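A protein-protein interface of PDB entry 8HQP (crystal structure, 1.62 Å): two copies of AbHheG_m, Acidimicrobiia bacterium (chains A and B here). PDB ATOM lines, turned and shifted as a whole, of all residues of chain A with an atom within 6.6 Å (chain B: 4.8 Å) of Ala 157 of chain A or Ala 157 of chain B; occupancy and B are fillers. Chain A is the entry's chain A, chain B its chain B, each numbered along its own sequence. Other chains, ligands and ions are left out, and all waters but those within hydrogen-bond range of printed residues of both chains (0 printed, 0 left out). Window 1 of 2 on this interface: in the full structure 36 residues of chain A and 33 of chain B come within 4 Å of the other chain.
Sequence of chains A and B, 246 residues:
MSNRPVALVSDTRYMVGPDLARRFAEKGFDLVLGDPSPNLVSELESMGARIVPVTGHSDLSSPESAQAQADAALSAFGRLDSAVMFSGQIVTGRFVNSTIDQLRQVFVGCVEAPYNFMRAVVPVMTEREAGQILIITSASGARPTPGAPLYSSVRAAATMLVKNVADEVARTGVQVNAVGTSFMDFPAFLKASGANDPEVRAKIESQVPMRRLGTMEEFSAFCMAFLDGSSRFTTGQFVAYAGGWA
Of the printed residues of chain B, Ala 157 of chain A touches Ser 153 and Ala 157.
Of chain A, only Ser 153 and Ala 157 come within 4 Å of Ala 157 of chain B.
Printed residues of chain B within 4 Å of Leu 161 of chain A: Ser 153.
Printed residues of chain A within 4 Å of Met 160 of chain B: Gly 141, Ser 152, Ser 153 and Ala 156.
The nearest residue of chain B that does not touch Ala 157 of chain A is Val 154 of chain B (4.5 Å).
Printed residues of chain B that touch a printed residue of chain A: Ser 153, Ala 156, Ala 157, Met 160 and Leu 161.
Hydrophobic or aromatic side chains of chain B that line the printed part of chain A: Ala 156, Ala 157, Met 160 and Leu 161.
Of the 15 printed residues of chain A, 7 touch a printed residue of chain B.
Among the printed residues, no Asp or Glu carboxylate lies within 4 Å of a Lys or Arg side-chain nitrogen of the other chain.
Among the printed residues, pairs that only touch across the chains: Gly 141 of chain A with Met 160 of chain B, Ala 157 of chain A with Ser 153 of chain B, Ser 153 of chain A with Ala 157 of chain B, Ser 152 of chain A with Met 160 of chain B, Met 160 of chain A with Ser 153 of chain B, Ala 157 of chain A with Ala 157 of chain B, Met 160 of chain A with Ala 156 of chain B, Ala 156 of chain A with Met 160 of chain B and Ser 153 of chain A with Met 160 of chain B.
Ser 153 of chain A touches Ala 157 of chain B, and with the chains exchanged Ala 157 of chain A touches Ser 153 of chain B.
Ser 153 of chain A touches Met 160 of chain B, and with the chains exchanged Met 160 of chain A touches Ser 153 of chain B.
Ser 153 of chain A touches Leu 161 of chain B, and with the chains exchanged Leu 161 of chain A touches Ser 153 of chain B.
Ala 157 of chain B touches its own counterpart, Ala 157 of chain A.
10 positions are printed for both chains.
Of the 11 pairs that touch across the chains among the printed residues, 9 have their exchanged pair printed and touching as well.
The backbone NH of Leu 161 of chain B sits close to the side-chain hydroxyl of Ser 153 of chain A, at 3.4 Å.
OG of Ser 153 of chain B lies close to N of Leu 161 of chain A (3.2 Å).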
ATOM      1  N   PHE A 107     -24.670  -9.953   3.301  1.00  0.00           N
ATOM      2  CA  PHE A 107     -23.492 -10.150   2.466  1.00  0.00           C
ATOM      3  C   PHE A 107     -22.224  -9.761   3.219  1.00  0.00           C
ATOM      4  O   PHE A 107     -21.199 -10.448   3.132  1.00  0.00           O
ATOM      5  CB  PHE A 107     -23.618  -9.321   1.187  1.00  0.00           C
ATOM      6  CG  PHE A 107     -22.373  -9.316   0.349  1.00  0.00           C
ATOM      7  CD1 PHE A 107     -22.001 -10.443  -0.364  1.00  0.00           C
ATOM      8  CD2 PHE A 107     -21.554  -8.203   0.310  1.00  0.00           C
ATOM      9  CE1 PHE A 107     -20.851 -10.446  -1.130  1.00  0.00           C
ATOM     10  CE2 PHE A 107     -20.404  -8.202  -0.452  1.00  0.00           C
ATOM     11  CZ  PHE A 107     -20.052  -9.324  -1.173  1.00  0.00           C
ATOM     12  N   CYS A 110     -21.702 -12.518   6.068  1.00  0.00           N
ATOM     13  CA  CYS A 110     -21.548 -13.892   5.592  1.00  0.00           C
ATOM     14  C   CYS A 110     -20.472 -14.073   4.532  1.00  0.00           C
ATOM     15  O   CYS A 110     -19.956 -15.188   4.388  1.00  0.00           O
ATOM     16  CB  CYS A 110     -22.876 -14.442   5.062  1.00  0.00           C
ATOM     17  SG  CYS A 110     -24.188 -14.462   6.318  1.00  0.00           S
ATOM     18  N   VAL A 111     -20.147 -13.037   3.754  1.00  0.00           N
ATOM     19  CA  VAL A 111     -19.232 -13.167   2.626  1.00  0.00           C
ATOM     20  C   VAL A 111     -17.994 -12.292   2.789  1.00  0.00           C
ATOM     21  O   VAL A 111     -16.867 -12.759   2.602  1.00  0.00           O
ATOM     22  CB  VAL A 111     -19.935 -12.867   1.285  1.00  0.00           C
ATOM     23  CG1 VAL A 111     -19.017 -13.264   0.134  1.00  0.00           C
ATOM     24  CG2 VAL A 111     -21.243 -13.634   1.190  1.00  0.00           C
ATOM     25  N   GLY A 141     -27.076 -22.146   3.244  1.00  0.00           N
ATOM     26  CA  GLY A 141     -26.752 -21.937   1.845  1.00  0.00           C
ATOM     27  C   GLY A 141     -26.853 -23.175   0.974  1.00  0.00           C
ATOM     28  O   GLY A 141     -26.776 -23.046  -0.251  1.00  0.00           O
ATOM     29  N   SER A 152     -29.784 -17.355   3.145  1.00  0.00           N
ATOM     30  CA  SER A 152     -29.422 -18.580   2.442  1.00  0.00           C
ATOM     31  C   SER A 152     -28.623 -18.277   1.178  1.00  0.00           C
ATOM     32  O   SER A 152     -27.636 -18.957   0.882  1.00  0.00           O
ATOM     33  CB  SER A 152     -30.688 -19.372   2.110  1.00  0.00           C
ATOM     34  OG  SER A 152     -30.421 -20.420   1.194  1.00  0.00           O
ATOM     35  N   SER A 153     -29.030 -17.247   0.428  1.00  0.00           N
ATOM     36  CA  SER A 153     -28.337 -16.904  -0.812  1.00  0.00           C
ATOM     37  C   SER A 153     -26.885 -16.513  -0.558  1.00  0.00           C
ATOM     38  O   SER A 153     -25.980 -16.991  -1.253  1.00  0.00           O
ATOM     39  CB  SER A 153     -29.080 -15.780  -1.534  1.00  0.00           C
ATOM     40  OG  SER A 153     -30.472 -16.024  -1.525  1.00  0.00           O
ATOM     41  N   VAL A 154     -26.632 -15.640   0.423  1.00  0.00           N
ATOM     42  CA  VAL A 154     -25.249 -15.203   0.631  1.00  0.00           C
ATOM     43  C   VAL A 154     -24.410 -16.300   1.280  1.00  0.00           C
ATOM     44  O   VAL A 154     -23.198 -16.385   1.039  1.00  0.00           O
ATOM     45  CB  VAL A 154     -25.185 -13.895   1.444  1.00  0.00           C
ATOM     46  CG1 VAL A 154     -25.843 -12.759   0.665  1.00  0.00           C
ATOM     47  CG2 VAL A 154     -25.793 -14.064   2.838  1.00  0.00           C
ATOM     48  N   ARG A 155     -25.014 -17.155   2.109  1.00  0.00           N
ATOM     49  CA  ARG A 155     -24.260 -18.285   2.642  1.00  0.00           C
ATOM     50  C   ARG A 155     -23.778 -19.192   1.516  1.00  0.00           C
ATOM     51  O   ARG A 155     -22.678 -19.752   1.583  1.00  0.00           O
ATOM     52  CB  ARG A 155     -25.111 -19.064   3.644  1.00  0.00           C
ATOM     53  CG  ARG A 155     -25.307 -18.344   4.968  1.00  0.00           C
ATOM     54  CD  ARG A 155     -24.015 -18.184   5.766  1.00  0.00           C
ATOM     55  NE  ARG A 155     -24.318 -17.892   7.164  1.00  0.00           N
ATOM     56  CZ  ARG A 155     -23.434 -17.491   8.069  1.00  0.00           C
ATOM     57  NH1 ARG A 155     -22.155 -17.344   7.769  1.00  0.00           N
ATOM     58  NH2 ARG A 155     -23.850 -17.217   9.305  1.00  0.00           N
ATOM     59  N   ALA A 156     -24.583 -19.333   0.460  1.00  0.00           N
ATOM     60  CA  ALA A 156     -24.156 -20.106  -0.701  1.00  0.00           C
ATOM     61  C   ALA A 156     -22.938 -19.481  -1.374  1.00  0.00           C
ATOM     62  O   ALA A 156     -22.061 -20.197  -1.864  1.00  0.00           O
ATOM     63  CB  ALA A 156     -25.309 -20.228  -1.697  1.00  0.00           C
ATOM     64  N   ALA A 157     -22.873 -18.145  -1.428  1.00  0.00           N
ATOM     65  CA  ALA A 157     -21.691 -17.493  -1.989  1.00  0.00           C
ATOM     66  C   ALA A 157     -20.456 -17.776  -1.148  1.00  0.00           C
ATOM     67  O   ALA A 157     -19.359 -17.963  -1.688  1.00  0.00           O
ATOM     68  CB  ALA A 157     -21.911 -15.983  -2.106  1.00  0.00           C
ATOM     69  N   ALA A 158     -20.609 -17.782   0.179  1.00  0.00           N
ATOM     70  CA  ALA A 158     -19.474 -18.044   1.056  1.00  0.00           C
ATOM     71  C   ALA A 158     -18.913 -19.438   0.814  1.00  0.00           C
ATOM     72  O   ALA A 158     -17.696 -19.617   0.692  1.00  0.00           O
ATOM     73  CB  ALA A 158     -19.892 -17.878   2.520  1.00  0.00           C
ATOM     74  N   THR A 159     -19.792 -20.439   0.717  1.00  0.00           N
ATOM     75  CA  THR A 159     -19.325 -21.805   0.495  1.00  0.00           C
ATOM     76  C   THR A 159     -18.678 -21.945  -0.873  1.00  0.00           C
ATOM     77  O   THR A 159     -17.649 -22.617  -1.012  1.00  0.00           O
ATOM     78  CB  THR A 159     -20.471 -22.803   0.653  1.00  0.00           C
ATOM     79  OG1 THR A 159     -20.845 -22.881   2.033  1.00  0.00           O
ATOM     80  CG2 THR A 159     -20.021 -24.188   0.209  1.00  0.00           C
ATOM     81  N   MET A 160     -19.266 -21.326  -1.900  1.00  0.00           N
ATOM     82  CA  MET A 160     -18.629 -21.358  -3.211  1.00  0.00           C
ATOM     83  C   MET A 160     -17.308 -20.595  -3.202  1.00  0.00           C
ATOM     84  O   MET A 160     -16.369 -20.982  -3.910  1.00  0.00           O
ATOM     85  CB  MET A 160     -19.584 -20.813  -4.270  1.00  0.00           C
ATOM     86  CG  MET A 160     -19.187 -21.105  -5.733  1.00  0.00           C
ATOM     87  SD  MET A 160     -18.517 -22.756  -6.098  1.00  0.00           S
ATOM     88  CE  MET A 160     -20.011 -23.743  -6.145  1.00  0.00           C
ATOM     89  N   LEU A 161     -17.202 -19.525  -2.403  1.00  0.00           N
ATOM     90  CA  LEU A 161     -15.921 -18.829  -2.299  1.00  0.00           C
ATOM     91  C   LEU A 161     -14.852 -19.748  -1.731  1.00  0.00           C
ATOM     92  O   LEU A 161     -13.735 -19.817  -2.251  1.00  0.00           O
ATOM     93  CB  LEU A 161     -16.051 -17.571  -1.441  1.00  0.00           C
ATOM     94  CG  LEU A 161     -14.786 -16.704  -1.385  1.00  0.00           C
ATOM     95  CD1 LEU A 161     -14.373 -16.232  -2.778  1.00  0.00           C
ATOM     96  CD2 LEU A 161     -14.929 -15.535  -0.417  1.00  0.00           C
ATOM     97  N   VAL A 162     -15.187 -20.470  -0.658  1.00  0.00           N
ATOM     98  CA  VAL A 162     -14.258 -21.440  -0.081  1.00  0.00           C
ATOM     99  C   VAL A 162     -13.832 -22.465  -1.126  1.00  0.00           C
ATOM    100  O   VAL A 162     -12.645 -22.782  -1.262  1.00  0.00           O
ATOM    101  CB  VAL A 162     -14.890 -22.110   1.151  1.00  0.00           C
ATOM    102  CG1 VAL A 162     -14.148 -23.393   1.509  1.00  0.00           C
ATOM    103  CG2 VAL A 162     -14.901 -21.145   2.310  1.00  0.00           C
ATOM    104  N   VAL B 111     -25.823 -10.144  -8.115  1.00  0.00           N
ATOM    105  CA  VAL B 111     -26.799 -10.468  -7.078  1.00  0.00           C
ATOM    106  C   VAL B 111     -27.790  -9.332  -6.848  1.00  0.00           C
ATOM    107  O   VAL B 111     -29.002  -9.559  -6.783  1.00  0.00           O
ATOM    108  CB  VAL B 111     -26.113 -10.871  -5.755  1.00  0.00           C
ATOM    109  CG1 VAL B 111     -27.150 -11.430  -4.794  1.00  0.00           C
ATOM    110  CG2 VAL B 111     -25.041 -11.921  -6.017  1.00  0.00           C
ATOM    111  N   SER B 153     -18.279 -17.113  -7.073  1.00  0.00           N
ATOM    112  CA  SER B 153     -18.894 -17.121  -5.752  1.00  0.00           C
ATOM    113  C   SER B 153     -20.205 -16.340  -5.733  1.00  0.00           C
ATOM    114  O   SER B 153     -21.218 -16.830  -5.220  1.00  0.00           O
ATOM    115  CB  SER B 153     -17.907 -16.567  -4.734  1.00  0.00           C
ATOM    116  OG  SER B 153     -16.729 -17.350  -4.768  1.00  0.00           O
ATOM    117  N   VAL B 154     -20.218 -15.125  -6.291  1.00  0.00           N
ATOM    118  CA  VAL B 154     -21.456 -14.347  -6.230  1.00  0.00           C
ATOM    119  C   VAL B 154     -22.498 -14.893  -7.202  1.00  0.00           C
ATOM    120  O   VAL B 154     -23.701 -14.754  -6.959  1.00  0.00           O
ATOM    121  CB  VAL B 154     -21.202 -12.842  -6.457  1.00  0.00           C
ATOM    122  CG1 VAL B 154     -20.369 -12.263  -5.307  1.00  0.00           C
ATOM    123  CG2 VAL B 154     -20.538 -12.592  -7.796  1.00  0.00           C
ATOM    124  N   ARG B 155     -22.074 -15.500  -8.320  1.00  0.00           N
ATOM    125  CA  ARG B 155     -23.049 -16.133  -9.209  1.00  0.00           C
ATOM    126  C   ARG B 155     -23.789 -17.252  -8.485  1.00  0.00           C
ATOM    127  O   ARG B 155     -24.983 -17.475  -8.721  1.00  0.00           O
ATOM    128  CB  ARG B 155     -22.370 -16.672 -10.471  1.00  0.00           C
ATOM    129  CG  ARG B 155     -21.928 -15.610 -11.485  1.00  0.00           C
ATOM    130  CD  ARG B 155     -23.068 -14.748 -12.039  1.00  0.00           C
ATOM    131  NE  ARG B 155     -22.662 -14.146 -13.307  1.00  0.00           N
ATOM    132  CZ  ARG B 155     -23.380 -13.279 -14.010  1.00  0.00           C
ATOM    133  NH1 ARG B 155     -24.567 -12.870 -13.601  1.00  0.00           N
ATOM    134  NH2 ARG B 155     -22.888 -12.809 -15.156  1.00  0.00           N
ATOM    135  N   ALA B 156     -23.089 -17.967  -7.599  1.00  0.00           N
ATOM    136  CA  ALA B 156     -23.728 -18.991  -6.776  1.00  0.00           C
ATOM    137  C   ALA B 156     -24.780 -18.386  -5.854  1.00  0.00           C
ATOM    138  O   ALA B 156     -25.811 -19.013  -5.584  1.00  0.00           O
ATOM    139  CB  ALA B 156     -22.668 -19.746  -5.968  1.00  0.00           C
ATOM    140  N   ALA B 157     -24.532 -17.176  -5.343  1.00  0.00           N
ATOM    141  CA  ALA B 157     -25.551 -16.506  -4.543  1.00  0.00           C
ATOM    142  C   ALA B 157     -26.790 -16.202  -5.374  1.00  0.00           C
ATOM    143  O   ALA B 157     -27.920 -16.375  -4.903  1.00  0.00           O
ATOM    144  CB  ALA B 157     -24.989 -15.218  -3.937  1.00  0.00           C
ATOM    145  N   ALA B 158     -26.597 -15.756  -6.619  1.00  0.00           N
ATOM    146  CA  ALA B 158     -27.737 -15.423  -7.468  1.00  0.00           C
ATOM    147  C   ALA B 158     -28.607 -16.645  -7.728  1.00  0.00           C
ATOM    148  O   ALA B 158     -29.839 -16.563  -7.667  1.00  0.00           O
ATOM    149  CB  ALA B 158     -27.253 -14.816  -8.785  1.00  0.00           C
ATOM    150  N   THR B 159     -27.984 -17.788  -8.022  1.00  0.00           N
ATOM    151  CA  THR B 159     -28.761 -18.999  -8.272  1.00  0.00           C
ATOM    152  C   THR B 159     -29.488 -19.456  -7.015  1.00  0.00           C
ATOM    153  O   THR B 159     -30.663 -19.836  -7.079  1.00  0.00           O
ATOM    154  CB  THR B 159     -27.856 -20.114  -8.793  1.00  0.00           C
ATOM    155  OG1 THR B 159     -27.214 -19.692 -10.003  1.00  0.00           O
ATOM    156  CG2 THR B 159     -28.661 -21.379  -9.052  1.00  0.00           C
ATOM    157  N   MET B 160     -28.815 -19.425  -5.862  1.00  0.00           N
ATOM    158  CA  MET B 160     -29.517 -19.785  -4.633  1.00  0.00           C
ATOM    159  C   MET B 160     -30.612 -18.789  -4.287  1.00  0.00           C
ATOM    160  O   MET B 160     -31.639 -19.184  -3.724  1.00  0.00           O
ATOM    161  CB  MET B 160     -28.538 -19.970  -3.478  1.00  0.00           C
ATOM    162  CG  MET B 160     -29.224 -20.521  -2.221  1.00  0.00           C
ATOM    163  SD  MET B 160     -30.035 -22.120  -2.464  1.00  0.00           S
ATOM    164  CE  MET B 160     -28.619 -23.163  -2.803  1.00  0.00           C
ATOM    165  N   LEU B 161     -30.427 -17.507  -4.613  1.00  0.00           N
ATOM    166  CA  LEU B 161     -31.502 -16.547  -4.397  1.00  0.00           C
ATOM    167  C   LEU B 161     -32.727 -16.919  -5.222  1.00  0.00           C
ATOM    168  O   LEU B 161     -33.854 -16.928  -4.714  1.00  0.00           O
ATOM    169  CB  LEU B 161     -31.038 -15.134  -4.751  1.00  0.00           C
ATOM    170  CG  LEU B 161     -32.134 -14.090  -4.505  1.00  0.00           C
ATOM    171  CD1 LEU B 161     -32.596 -14.131  -3.051  1.00  0.00           C
ATOM    172  CD2 LEU B 161     -31.711 -12.682  -4.927  1.00  0.00           C
